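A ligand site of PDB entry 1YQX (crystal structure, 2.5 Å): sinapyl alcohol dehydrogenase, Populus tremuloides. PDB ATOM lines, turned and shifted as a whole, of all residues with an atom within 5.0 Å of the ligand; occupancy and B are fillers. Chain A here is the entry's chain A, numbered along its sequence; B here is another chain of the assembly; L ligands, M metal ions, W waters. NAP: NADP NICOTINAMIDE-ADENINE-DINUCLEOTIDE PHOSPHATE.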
ATOM      1  N   CYS A  54      22.729   1.199  23.631  1.00  0.00           N
ATOM      2  CA  CYS A  54      23.758   0.958  24.627  1.00  0.00           C
ATOM      3  C   CYS A  54      23.099   0.455  25.903  1.00  0.00           C
ATOM      4  O   CYS A  54      21.958   0.805  26.186  1.00  0.00           O
ATOM      5  CB  CYS A  54      24.523   2.261  24.897  1.00  0.00           C
ATOM      6  SG  CYS A  54      25.815   2.151  26.172  1.00  0.00           S
ATOM      7  N   HIS A  55      23.820  -0.357  26.679  1.00  0.00           N
ATOM      8  CA  HIS A  55      23.240  -0.873  27.916  1.00  0.00           C
ATOM      9  C   HIS A  55      22.925   0.262  28.900  1.00  0.00           C
ATOM     10  O   HIS A  55      22.150   0.085  29.822  1.00  0.00           O
ATOM     11  CB  HIS A  55      24.163  -1.900  28.561  1.00  0.00           C
ATOM     12  CG  HIS A  55      23.474  -2.827  29.517  1.00  0.00           C
ATOM     13  ND1 HIS A  55      23.332  -4.179  29.277  1.00  0.00           N
ATOM     14  CD2 HIS A  55      22.924  -2.608  30.732  1.00  0.00           C
ATOM     15  CE1 HIS A  55      22.742  -4.751  30.309  1.00  0.00           C
ATOM     16  NE2 HIS A  55      22.483  -3.823  31.200  1.00  0.00           N
ATOM     17  N   SER A  56      23.525   1.429  28.671  1.00  0.00           N
ATOM     18  CA  SER A  56      23.280   2.596  29.529  1.00  0.00           C
ATOM     19  C   SER A  56      21.865   3.105  29.318  1.00  0.00           C
ATOM     20  O   SER A  56      21.268   3.684  30.211  1.00  0.00           O
ATOM     21  CB  SER A  56      24.266   3.719  29.216  1.00  0.00           C
ATOM     22  OG  SER A  56      25.523   3.456  29.806  1.00  0.00           O
ATOM     23  N   HIS A  59      19.909   0.749  31.654  1.00  0.00           N
ATOM     24  CA  HIS A  59      20.077   1.120  33.063  1.00  0.00           C
ATOM     25  C   HIS A  59      19.235   2.359  33.380  1.00  0.00           C
ATOM     26  O   HIS A  59      18.533   2.390  34.382  1.00  0.00           O
ATOM     27  CB  HIS A  59      21.542   1.431  33.401  1.00  0.00           C
ATOM     28  CG  HIS A  59      22.478   0.260  33.341  1.00  0.00           C
ATOM     29  ND1 HIS A  59      22.332  -0.861  34.138  1.00  0.00           N
ATOM     30  CD2 HIS A  59      23.623   0.069  32.640  1.00  0.00           C
ATOM     31  CE1 HIS A  59      23.338  -1.687  33.927  1.00  0.00           C
ATOM     32  NE2 HIS A  59      24.139  -1.140  33.032  1.00  0.00           N
ATOM     33  N   TRP A  65      20.307   3.382  38.486  1.00  0.00           N
ATOM     34  CA  TRP A  65      21.181   4.208  39.293  1.00  0.00           C
ATOM     35  C   TRP A  65      20.426   5.215  40.145  1.00  0.00           C
ATOM     36  O   TRP A  65      21.032   5.931  40.941  1.00  0.00           O
ATOM     37  CB  TRP A  65      22.194   4.922  38.401  1.00  0.00           C
ATOM     38  CG  TRP A  65      23.020   3.960  37.573  1.00  0.00           C
ATOM     39  CD1 TRP A  65      23.643   2.841  38.023  1.00  0.00           C
ATOM     40  CD2 TRP A  65      23.308   4.052  36.177  1.00  0.00           C
ATOM     41  NE1 TRP A  65      24.299   2.209  36.987  1.00  0.00           N
ATOM     42  CE2 TRP A  65      24.109   2.937  35.841  1.00  0.00           C
ATOM     43  CE3 TRP A  65      22.969   4.961  35.167  1.00  0.00           C
ATOM     44  CZ2 TRP A  65      24.584   2.705  34.546  1.00  0.00           C
ATOM     45  CZ3 TRP A  65      23.438   4.736  33.869  1.00  0.00           C
ATOM     46  CH2 TRP A  65      24.239   3.620  33.571  1.00  0.00           C
ATOM     47  N   CYS A 170      30.014   5.600  21.397  1.00  0.00           N
ATOM     48  CA  CYS A 170      30.077   5.467  22.838  1.00  0.00           C
ATOM     49  C   CYS A 170      30.832   4.196  23.235  1.00  0.00           C
ATOM     50  O   CYS A 170      31.857   4.259  23.919  1.00  0.00           O
ATOM     51  CB  CYS A 170      28.685   5.423  23.443  1.00  0.00           C
ATOM     52  SG  CYS A 170      28.719   5.219  25.229  1.00  0.00           S
ATOM     53  N   THR A 174      34.657   4.573  24.340  1.00  0.00           N
ATOM     54  CA  THR A 174      34.810   4.166  25.732  1.00  0.00           C
ATOM     55  C   THR A 174      35.868   3.109  26.029  1.00  0.00           C
ATOM     56  O   THR A 174      36.491   3.162  27.079  1.00  0.00           O
ATOM     57  CB  THR A 174      33.426   3.741  26.307  1.00  0.00           C
ATOM     58  OG1 THR A 174      32.605   4.906  26.446  1.00  0.00           O
ATOM     59  CG2 THR A 174      33.569   3.084  27.690  1.00  0.00           C
ATOM     60  N   GLY A 195      33.615  -9.592  29.512  1.00  0.00           N
ATOM     61  CA  GLY A 195      32.278  -9.350  28.984  1.00  0.00           C
ATOM     62  C   GLY A 195      32.262  -9.053  27.487  1.00  0.00           C
ATOM     63  O   GLY A 195      32.500  -7.921  27.069  1.00  0.00           O
ATOM     64  N   LEU A 196      31.973 -10.073  26.680  1.00  0.00           N
ATOM     65  CA  LEU A 196      31.939  -9.898  25.240  1.00  0.00           C
ATOM     66  C   LEU A 196      30.579  -9.355  24.784  1.00  0.00           C
ATOM     67  O   LEU A 196      29.845 -10.010  24.060  1.00  0.00           O
ATOM     68  CB  LEU A 196      32.272 -11.221  24.540  1.00  0.00           C
ATOM     69  CG  LEU A 196      32.660 -11.167  23.053  1.00  0.00           C
ATOM     70  CD1 LEU A 196      33.950 -10.374  22.883  1.00  0.00           C
ATOM     71  CD2 LEU A 196      32.847 -12.593  22.521  1.00  0.00           C
ATOM     72  N   GLY A 197      30.258  -8.155  25.230  1.00  0.00           N
ATOM     73  CA  GLY A 197      29.014  -7.525  24.843  1.00  0.00           C
ATOM     74  C   GLY A 197      29.272  -6.367  23.905  1.00  0.00           C
ATOM     75  O   GLY A 197      30.243  -6.372  23.149  1.00  0.00           O
ATOM     76  N   GLY A 198      28.407  -5.361  23.950  1.00  0.00           N
ATOM     77  CA  GLY A 198      28.569  -4.207  23.090  1.00  0.00           C
ATOM     78  C   GLY A 198      29.973  -3.629  23.156  1.00  0.00           C
ATOM     79  O   GLY A 198      30.717  -3.697  22.178  1.00  0.00           O
ATOM     80  N   LEU A 199      30.324  -3.072  24.310  1.00  0.00           N
ATOM     81  CA  LEU A 199      31.647  -2.507  24.505  1.00  0.00           C
ATOM     82  C   LEU A 199      32.737  -3.563  24.377  1.00  0.00           C
ATOM     83  O   LEU A 199      33.790  -3.318  23.793  1.00  0.00           O
ATOM     84  CB  LEU A 199      31.748  -1.818  25.880  1.00  0.00           C
ATOM     85  CG  LEU A 199      31.311  -0.343  25.906  1.00  0.00           C
ATOM     86  CD1 LEU A 199      29.813  -0.239  25.633  1.00  0.00           C
ATOM     87  CD2 LEU A 199      31.653   0.292  27.257  1.00  0.00           C
ATOM     88  N   GLY A 200      32.452  -4.750  24.915  1.00  0.00           N
ATOM     89  CA  GLY A 200      33.391  -5.864  24.892  1.00  0.00           C
ATOM     90  C   GLY A 200      33.950  -6.274  23.551  1.00  0.00           C
ATOM     91  O   GLY A 200      35.175  -6.321  23.393  1.00  0.00           O
ATOM     92  N   ILE A 217      37.341 -12.699  28.689  1.00  0.00           N
ATOM     93  CA  ILE A 217      36.810 -13.374  29.866  1.00  0.00           C
ATOM     94  C   ILE A 217      35.303 -13.216  29.768  1.00  0.00           C
ATOM     95  O   ILE A 217      34.789 -12.102  29.801  1.00  0.00           O
ATOM     96  CB  ILE A 217      37.333 -12.753  31.185  1.00  0.00           C
ATOM     97  CG1 ILE A 217      38.860 -12.921  31.282  1.00  0.00           C
ATOM     98  CG2 ILE A 217      36.684 -13.449  32.372  1.00  0.00           C
ATOM     99  CD1 ILE A 217      39.654 -11.895  30.489  1.00  0.00           C
ATOM    100  N   SER A 218      34.612 -14.337  29.654  1.00  0.00           N
ATOM    101  CA  SER A 218      33.162 -14.351  29.477  1.00  0.00           C
ATOM    102  C   SER A 218      32.401 -15.351  30.341  1.00  0.00           C
ATOM    103  O   SER A 218      32.993 -16.291  30.895  1.00  0.00           O
ATOM    104  CB  SER A 218      32.859 -14.631  28.001  1.00  0.00           C
ATOM    105  OG  SER A 218      31.494 -14.929  27.797  1.00  0.00           O
ATOM    106  N   THR A 219      31.084 -15.163  30.462  1.00  0.00           N
ATOM    107  CA  THR A 219      30.265 -16.096  31.228  1.00  0.00           C
ATOM    108  C   THR A 219      29.431 -16.942  30.263  1.00  0.00           C
ATOM    109  O   THR A 219      28.734 -17.862  30.682  1.00  0.00           O
ATOM    110  CB  THR A 219      29.276 -15.396  32.171  1.00  0.00           C
ATOM    111  OG1 THR A 219      28.322 -14.658  31.389  1.00  0.00           O
ATOM    112  CG2 THR A 219      29.999 -14.471  33.131  1.00  0.00           C
ATOM    113  N   SER A 220      29.510 -16.610  28.972  1.00  0.00           N
ATOM    114  CA  SER A 220      28.753 -17.314  27.933  1.00  0.00           C
ATOM    115  C   SER A 220      29.607 -18.185  27.014  1.00  0.00           C
ATOM    116  O   SER A 220      30.036 -17.747  25.943  1.00  0.00           O
ATOM    117  CB  SER A 220      28.011 -16.284  27.074  1.00  0.00           C
ATOM    118  OG  SER A 220      27.158 -15.486  27.868  1.00  0.00           O
ATOM    119  N   LYS A 223      29.982 -18.121  23.078  1.00  0.00           N
ATOM    120  CA  LYS A 223      30.568 -17.000  22.335  1.00  0.00           C
ATOM    121  C   LYS A 223      32.031 -17.309  22.053  1.00  0.00           C
ATOM    122  O   LYS A 223      32.702 -16.562  21.338  1.00  0.00           O
ATOM    123  CB  LYS A 223      30.484 -15.702  23.149  1.00  0.00           C
ATOM    124  CG  LYS A 223      29.097 -15.097  23.283  1.00  0.00           C
ATOM    125  CD  LYS A 223      29.178 -13.805  24.088  1.00  0.00           C
ATOM    126  CE  LYS A 223      27.821 -13.292  24.514  1.00  0.00           C
ATOM    127  NZ  LYS A 223      27.946 -12.043  25.323  1.00  0.00           N
ATOM    128  N   THR A 258      33.981  -4.591  31.125  1.00  0.00           N
ATOM    129  CA  THR A 258      32.784  -3.947  30.619  1.00  0.00           C
ATOM    130  C   THR A 258      31.515  -4.483  31.254  1.00  0.00           C
ATOM    131  O   THR A 258      30.426  -4.007  30.943  1.00  0.00           O
ATOM    132  CB  THR A 258      32.669  -4.113  29.101  1.00  0.00           C
ATOM    133  OG1 THR A 258      32.235  -5.445  28.801  1.00  0.00           O
ATOM    134  CG2 THR A 258      34.032  -3.880  28.435  1.00  0.00           C
ATOM    135  N   VAL A 259      31.656  -5.476  32.143  1.00  0.00           N
ATOM    136  CA  VAL A 259      30.526  -6.115  32.802  1.00  0.00           C
ATOM    137  C   VAL A 259      29.507  -5.146  33.402  1.00  0.00           C
ATOM    138  O   VAL A 259      29.843  -4.288  34.225  1.00  0.00           O
ATOM    139  CB  VAL A 259      31.008  -7.117  33.889  1.00  0.00           C
ATOM    140  CG1 VAL A 259      29.815  -7.712  34.637  1.00  0.00           C
ATOM    141  CG2 VAL A 259      31.803  -8.238  33.243  1.00  0.00           C
ATOM    142  N   SER A 260      28.252  -5.317  33.000  1.00  0.00           N
ATOM    143  CA  SER A 260      27.152  -4.468  33.433  1.00  0.00           C
ATOM    144  C   SER A 260      26.471  -4.851  34.749  1.00  0.00           C
ATOM    145  O   SER A 260      25.489  -4.246  35.142  1.00  0.00           O
ATOM    146  CB  SER A 260      26.099  -4.384  32.336  1.00  0.00           C
ATOM    147  OG  SER A 260      25.659  -5.678  31.964  1.00  0.00           O
ATOM    148  N   ALA A 261      26.987  -5.836  35.450  1.00  0.00           N
ATOM    149  CA  ALA A 261      26.381  -6.230  36.703  1.00  0.00           C
ATOM    150  C   ALA A 261      27.475  -6.489  37.715  1.00  0.00           C
ATOM    151  O   ALA A 261      28.648  -6.584  37.360  1.00  0.00           O
ATOM    152  CB  ALA A 261      25.539  -7.462  36.508  1.00  0.00           C
ATOM    153  N   VAL A 262      27.090  -6.589  38.986  1.00  0.00           N
ATOM    154  CA  VAL A 262      28.068  -6.876  40.026  1.00  0.00           C
ATOM    155  C   VAL A 262      28.652  -8.231  39.650  1.00  0.00           C
ATOM    156  O   VAL A 262      27.929  -9.100  39.154  1.00  0.00           O
ATOM    157  CB  VAL A 262      27.412  -6.942  41.416  1.00  0.00           C
ATOM    158  CG1 VAL A 262      28.268  -7.761  42.376  1.00  0.00           C
ATOM    159  CG2 VAL A 262      27.234  -5.531  41.966  1.00  0.00           C
ATOM    160  N   HIS A 263      29.955  -8.392  39.869  1.00  0.00           N
ATOM    161  CA  HIS A 263      30.628  -9.642  39.560  1.00  0.00           C
ATOM    162  C   HIS A 263      31.919  -9.737  40.374  1.00  0.00           C
ATOM    163  O   HIS A 263      32.422  -8.728  40.846  1.00  0.00           O
ATOM    164  CB  HIS A 263      30.933  -9.702  38.047  1.00  0.00           C
ATOM    165  CG  HIS A 263      31.759  -8.562  37.563  1.00  0.00           C
ATOM    166  ND1 HIS A 263      31.323  -7.262  37.565  1.00  0.00           N
ATOM    167  CD2 HIS A 263      33.025  -8.523  37.071  1.00  0.00           C
ATOM    168  CE1 HIS A 263      32.271  -6.462  37.113  1.00  0.00           C
ATOM    169  NE2 HIS A 263      33.316  -7.205  36.801  1.00  0.00           N
ATOM    170  N   VAL A 281      34.919  -0.155  33.414  1.00  0.00           N
ATOM    171  CA  VAL A 281      34.260   0.682  32.434  1.00  0.00           C
ATOM    172  C   VAL A 281      32.752   0.401  32.516  1.00  0.00           C
ATOM    173  O   VAL A 281      31.922   1.270  32.247  1.00  0.00           O
ATOM    174  CB  VAL A 281      34.861   0.413  31.027  1.00  0.00           C
ATOM    175  CG1 VAL A 281      33.928  -0.453  30.178  1.00  0.00           C
ATOM    176  CG2 VAL A 281      35.199   1.712  30.354  1.00  0.00           C
ATOM    177  N   GLY A 282      32.402  -0.811  32.919  1.00  0.00           N
ATOM    178  CA  GLY A 282      31.003  -1.155  33.057  1.00  0.00           C
ATOM    179  C   GLY A 282      30.443  -0.453  34.276  1.00  0.00           C
ATOM    180  O   GLY A 282      31.208  -0.008  35.123  1.00  0.00           O
ATOM    181  N   ALA A 283      29.125  -0.354  34.391  1.00  0.00           N
ATOM    182  CA  ALA A 283      28.543   0.331  35.542  1.00  0.00           C
ATOM    183  C   ALA A 283      27.449  -0.450  36.257  1.00  0.00           C
ATOM    184  O   ALA A 283      26.274  -0.294  35.978  1.00  0.00           O
ATOM    185  CB  ALA A 283      28.003   1.699  35.106  1.00  0.00           C
ATOM    186  N   PRO A 284      27.837  -1.308  37.207  1.00  0.00           N
ATOM    187  CA  PRO A 284      26.839  -2.096  37.934  1.00  0.00           C
ATOM    188  C   PRO A 284      25.999  -1.174  38.804  1.00  0.00           C
ATOM    189  O   PRO A 284      26.460  -0.108  39.227  1.00  0.00           O
ATOM    190  CB  PRO A 284      27.693  -3.046  38.770  1.00  0.00           C
ATOM    191  CG  PRO A 284      28.958  -3.161  37.974  1.00  0.00           C
ATOM    192  CD  PRO A 284      29.196  -1.747  37.562  1.00  0.00           C
ATOM    193  N   SER A 305      37.084   4.530  33.836  1.00  0.00           N
ATOM    194  CA  SER A 305      37.142   5.396  32.677  1.00  0.00           C
ATOM    195  C   SER A 305      35.730   5.593  32.101  1.00  0.00           C
ATOM    196  O   SER A 305      34.917   4.655  32.065  1.00  0.00           O
ATOM    197  CB  SER A 305      38.056   4.806  31.612  1.00  0.00           C
ATOM    198  OG  SER A 305      38.145   5.677  30.502  1.00  0.00           O
ATOM    199  N   GLY A 306      35.461   6.823  31.685  1.00  0.00           N
ATOM    200  CA  GLY A 306      34.168   7.157  31.109  1.00  0.00           C
ATOM    201  C   GLY A 306      34.347   7.744  29.725  1.00  0.00           C
ATOM    202  O   GLY A 306      35.055   8.742  29.571  1.00  0.00           O
ATOM    203  N   ILE A 307      33.701   7.130  28.731  1.00  0.00           N
ATOM    204  CA  ILE A 307      33.773   7.572  27.335  1.00  0.00           C
ATOM    205  C   ILE A 307      35.106   8.228  27.020  1.00  0.00           C
ATOM    206  O   ILE A 307      36.170   7.708  27.353  1.00  0.00           O
ATOM    207  CB  ILE A 307      32.642   8.580  27.007  1.00  0.00           C
ATOM    208  CG1 ILE A 307      32.629   9.705  28.055  1.00  0.00           C
ATOM    209  CG2 ILE A 307      31.303   7.867  26.946  1.00  0.00           C
ATOM    210  CD1 ILE A 307      31.558  10.757  27.814  1.00  0.00           C
ATOM    211  N   LEU A 344      18.369  -7.386  25.443  1.00  0.00           N
ATOM    212  CA  LEU A 344      19.657  -6.893  25.876  1.00  0.00           C
ATOM    213  C   LEU A 344      19.879  -7.290  27.315  1.00  0.00           C
ATOM    214  O   LEU A 344      20.935  -7.804  27.683  1.00  0.00           O
ATOM    215  CB  LEU A 344      19.720  -5.385  25.736  1.00  0.00           C
ATOM    216  CG  LEU A 344      21.137  -4.864  26.004  1.00  0.00           C
ATOM    217  CD1 LEU A 344      22.106  -5.470  24.982  1.00  0.00           C
ATOM    218  CD2 LEU A 344      21.124  -3.339  25.948  1.00  0.00           C
ATOM    219  N   ASN A 347      21.134 -10.792  27.682  1.00  0.00           N
ATOM    220  CA  ASN A 347      22.306 -11.209  26.907  1.00  0.00           C
ATOM    221  C   ASN A 347      21.916 -11.900  25.594  1.00  0.00           C
ATOM    222  O   ASN A 347      22.554 -12.871  25.180  1.00  0.00           O
ATOM    223  CB  ASN A 347      23.166 -12.155  27.776  1.00  0.00           C
ATOM    224  CG  ASN A 347      24.668 -11.980  27.567  1.00  0.00           C
ATOM    225  OD1 ASN A 347      25.488 -12.550  28.296  1.00  0.00           O
ATOM    226  ND2 ASN A 347      25.043 -11.182  26.578  1.00  0.00           N
ATOM    227  N   TYR A 351      25.926  -8.830  19.786  1.00  0.00           N
ATOM    228  CA  TYR A 351      26.684  -7.629  19.990  1.00  0.00           C
ATOM    229  C   TYR A 351      25.998  -6.293  20.066  1.00  0.00           C
ATOM    230  O   TYR A 351      25.980  -5.713  21.131  1.00  0.00           O
ATOM    231  CB  TYR A 351      27.883  -7.706  19.079  1.00  0.00           C
ATOM    232  CG  TYR A 351      28.568  -9.019  19.377  1.00  0.00           C
ATOM    233  CD1 TYR A 351      28.788  -9.978  18.383  1.00  0.00           C
ATOM    234  CD2 TYR A 351      28.862  -9.378  20.698  1.00  0.00           C
ATOM    235  CE1 TYR A 351      29.255 -11.252  18.684  1.00  0.00           C
ATOM    236  CE2 TYR A 351      29.324 -10.652  21.013  1.00  0.00           C
ATOM    237  CZ  TYR A 351      29.525 -11.577  20.003  1.00  0.00           C
ATOM    238  OH  TYR A 351      29.969 -12.836  20.325  1.00  0.00           O
ATOM    239  N   ARG A 352      25.385  -5.778  19.008  1.00  0.00           N
ATOM    240  CA  ARG A 352      24.766  -4.469  19.192  1.00  0.00           C
ATOM    241  C   ARG A 352      23.507  -4.169  18.397  1.00  0.00           C
ATOM    242  O   ARG A 352      23.459  -4.303  17.181  1.00  0.00           O
ATOM    243  CB  ARG A 352      25.807  -3.363  18.922  1.00  0.00           C
ATOM    244  CG  ARG A 352      26.332  -2.646  20.155  1.00  0.00           C
ATOM    245  CD  ARG A 352      25.405  -1.524  20.596  1.00  0.00           C
ATOM    246  NE  ARG A 352      26.051  -0.542  21.481  1.00  0.00           N
ATOM    247  CZ  ARG A 352      26.422  -0.772  22.735  1.00  0.00           C
ATOM    248  NH1 ARG A 352      26.221  -1.957  23.296  1.00  0.00           N
ATOM    249  NH2 ARG A 352      26.988   0.195  23.433  1.00  0.00           N
ATOM    250  N   ILE B 296      34.867   5.863  37.722  1.00  0.00           N
ATOM    251  CA  ILE B 296      34.497   6.272  36.379  1.00  0.00           C
ATOM    252  C   ILE B 296      34.251   7.775  36.308  1.00  0.00           C
ATOM    253  O   ILE B 296      34.792   8.473  35.442  1.00  0.00           O
ATOM    254  CB  ILE B 296      33.223   5.526  35.907  1.00  0.00           C
ATOM    255  CG1 ILE B 296      33.431   4.017  36.017  1.00  0.00           C
ATOM    256  CG2 ILE B 296      32.878   5.922  34.468  1.00  0.00           C
ATOM    257  CD1 ILE B 296      32.219   3.202  35.667  1.00  0.00           C
HETATM  258  PA  NAP L   1      25.902  -5.389  27.048  1.00  0.00           P
HETATM  259  O1A NAP L   1      24.837  -5.837  27.800  1.00  0.00           O
HETATM  260  O2A NAP L   1      25.925  -5.292  25.557  1.00  0.00           O
HETATM  261  O5B NAP L   1      27.245  -6.188  27.379  1.00  0.00           O
HETATM  262  C5B NAP L   1      27.514  -6.463  28.764  1.00  0.00           C
HETATM  263  C4B NAP L   1      28.369  -7.726  28.543  1.00  0.00           C
HETATM  264  O4B NAP L   1      28.759  -8.319  30.020  1.00  0.00           O
HETATM  265  C3B NAP L   1      27.358  -9.084  28.464  1.00  0.00           C
HETATM  266  O3B NAP L   1      27.623  -9.438  27.015  1.00  0.00           O
HETATM  267  C2B NAP L   1      27.950 -10.234  29.137  1.00  0.00           C
HETATM  268  O2B NAP L   1      29.171 -10.660  28.561  1.00  0.00           O
HETATM  269  C1B NAP L   1      28.470  -9.454  30.442  1.00  0.00           C
HETATM  270  N9A NAP L   1      27.489  -9.605  31.529  1.00  0.00           N
HETATM  271  C8A NAP L   1      26.152  -9.220  31.628  1.00  0.00           C
HETATM  272  N7A NAP L   1      25.596  -9.538  32.807  1.00  0.00           N
HETATM  273  C5A NAP L   1      26.639 -10.172  33.498  1.00  0.00           C
HETATM  274  C6A NAP L   1      26.672 -10.760  34.846  1.00  0.00           C
HETATM  275  N6A NAP L   1      25.666 -10.819  35.748  1.00  0.00           N
HETATM  276  N1A NAP L   1      27.919 -11.340  35.285  1.00  0.00           N
HETATM  277  C2A NAP L   1      29.060 -11.331  34.410  1.00  0.00           C
HETATM  278  N3A NAP L   1      29.039 -10.769  33.113  1.00  0.00           N
HETATM  279  C4A NAP L   1      27.816 -10.200  32.698  1.00  0.00           C
HETATM  280  O3  NAP L   1      26.289  -3.924  27.523  1.00  0.00           O
HETATM  281  PN  NAP L   1      27.142  -2.856  26.734  1.00  0.00           P
HETATM  282  O1N NAP L   1      28.578  -2.966  26.640  1.00  0.00           O
HETATM  283  O2N NAP L   1      26.366  -1.748  26.215  1.00  0.00           O
HETATM  284  O5D NAP L   1      27.332  -2.019  28.136  1.00  0.00           O
HETATM  285  C5D NAP L   1      28.091  -2.557  29.301  1.00  0.00           C
HETATM  286  C4D NAP L   1      28.192  -1.617  30.517  1.00  0.00           C
HETATM  287  O4D NAP L   1      29.083  -0.474  30.304  1.00  0.00           O
HETATM  288  C3D NAP L   1      26.876  -0.922  31.109  1.00  0.00           C
HETATM  289  O3D NAP L   1      26.885  -0.971  32.573  1.00  0.00           O
HETATM  290  C2D NAP L   1      26.972   0.485  30.608  1.00  0.00           C
HETATM  291  O2D NAP L   1      26.140   1.369  31.354  1.00  0.00           O
HETATM  292  C1D NAP L   1      28.395   0.746  30.759  1.00  0.00           C
HETATM  293  N1N NAP L   1      29.018   1.820  29.986  1.00  0.00           N
HETATM  294  C2N NAP L   1      29.943   2.719  30.598  1.00  0.00           C
HETATM  295  C3N NAP L   1      30.520   3.737  29.824  1.00  0.00           C
HETATM  296  C7N NAP L   1      31.508   4.676  30.503  1.00  0.00           C
HETATM  297  O7N NAP L   1      31.997   5.548  29.823  1.00  0.00           O
HETATM  298  N7N NAP L   1      31.799   4.530  31.764  1.00  0.00           N
HETATM  299  C4N NAP L   1      30.207   3.898  28.390  1.00  0.00           C
HETATM  300  C5N NAP L   1      29.271   2.976  27.820  1.00  0.00           C
HETATM  301  C6N NAP L   1      28.658   1.912  28.597  1.00  0.00           C
HETATM  302  P2B NAP L   1      29.566 -12.309  28.548  1.00  0.00           P
HETATM  303  O1X NAP L   1      30.922 -12.356  27.828  1.00  0.00           O
HETATM  304  O2X NAP L   1      29.637 -12.668  30.007  1.00  0.00           O
HETATM  305  O3X NAP L   1      28.495 -12.994  27.733  1.00  0.00           O
HETATM  306 ZN    ZN M   1      26.741   4.346  26.259  1.00  0.00          ZN
HETATM  307  O   HOH W   1      27.134   5.468  28.628  1.00  0.00           O
HETATM  308  O   HOH W   2      30.440  -5.385  26.414  1.00  0.00           O
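The backbone carbonyl oxygen of Ile 217 is in hydrogen-bond range of the backbone NH of Gly 195 (2.8 Å). OG of Ser 220 is in hydrogen-bond range of OD1 of Asn 347 (3.4 Å). NZ of Lys 223 lies within hydrogen-bond range of O of Leu 196. The backbone carbonyl oxygen of Cys 170 sits at hydrogen-bond distance from the side-chain hydroxyl of Thr 174 (2.7 Å). The side-chain hydroxyl of Thr 174 lies close to the backbone NH of Ile 307, at 3.4 Å. NZ of Lys 223 sits close to ND2 of Asn 347 (3.3 Å). OG of Ser 218 lies within hydrogen-bond range of N of Ser 220 (2.9 Å). The guanidinium group of Arg 352 sits close to the side-chain sulfur of Cys 54, at 3.6 Å.
O1X of the ligand lies within hydrogen-bond range of N of Leu 196 (2.8 Å). The backbone NH of His 55 is in hydrogen-bond range of an oxygen (O2N) of the ligand, at 2.9 Å. The side-chain hydroxyl of Ser 56 lies within hydrogen-bond range of an oxygen (O2D) of the ligand, at 2.7 Å. The guanidinium group (NH1) of Arg 352 lies within salt-bridge range of an oxygen (O2N) of the ligand (2.9 Å). O3D of the ligand lies within hydrogen-bond range of NE2 of His 59 (2.8 Å). The backbone NH of Ile 307 is in hydrogen-bond range of an oxygen (O7N) of the ligand, 2.6 Å away. OD1 of Asn 347 lies close to O3X of the ligand (3.1 Å). The backbone carbonyl oxygen (O) of Val 281 sits close to a nitrogen (N7N) of the ligand, 3.3 Å away. O of Ser 305 sits at hydrogen-bond distance from N7N of the ligand, 3.1 Å away. O3X of the ligand lies within salt-bridge range of NZ of Lys 223 (2.6 Å). O2X of the ligand is in hydrogen-bond range of N of Thr 219. An oxygen (O7N) of the ligand sits close to the side-chain hydroxyl (OG1) of Thr 174 (3.5 Å). An oxygen (O1A) of the ligand lies within hydrogen-bond range of a ring nitrogen (ND1) of His 55, 2.7 Å away. OG of Ser 220 lies within hydrogen-bond range of O3X of the ligand, 2.8 Å away. N of Ala 283 sits at hydrogen-bond distance from O3D of the ligand (3.0 Å). O2X of the ligand lies within hydrogen-bond range of OG1 of Thr 219. N of Gly 197 sits close to O3B of the ligand (3.4 Å). An oxygen (O1X) of the ligand sits at hydrogen-bond distance from the side-chain hydroxyl of Ser 218 (2.6 Å). O2A of the ligand lies within hydrogen-bond range of N of Gly 198 (3.0 Å). The backbone NH (N) of Leu 199 sits at hydrogen-bond distance from an oxygen (O1N) of the ligand (2.9 Å).
Cys 54 touches the ligand (SG to C6N, 3.7 Å). Trp 65 touches the ligand. Cys 170 touches the ligand (SG to C5N, 3.5 Å). CA of Gly 195 touches O2B of the ligand (3.4 Å). O of Thr 258 touches C5D of the ligand (3.2 Å). Val 259 touches the ligand (CG1 to N3A, 3.5 Å). CB of Ser 260 touches O3D of the ligand, at 3.5 Å. Ala 261 touches the ligand. CA of Gly 282 touches O4D of the ligand (3.4 Å). CA of Gly 306 touches O7N of the ligand (3.0 Å). Leu 344 touches the ligand (CD1 to O2A, 3.9 Å). CG2 of Ile 296 of chain B touches N7N of the ligand (3.2 Å). Hydrophobic or aromatic side chains that line the ligand: His 55, His 59, Trp 65, Leu 196, Leu 199, Val 259, Ala 261, Ala 283, Ile 307, Leu 344 and Ile 296 of chain B. Within 4 Å of the ligand: Cys 54, His 55, Ser 56, His 59, Trp 65, Cys 170, Thr 174, Gly 195, Leu 196, Gly 197, Gly 198, Leu 199, Ser 218, Thr 219, Ser 220, Lys 223, Thr 258, Val 259, Ser 260, Ala 261, Val 281, Gly 282, Ala 283, Ser 305, Gly 306, Ile 307, Leu 344, Asn 347, Arg 352 and Ile 296 of chain B.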
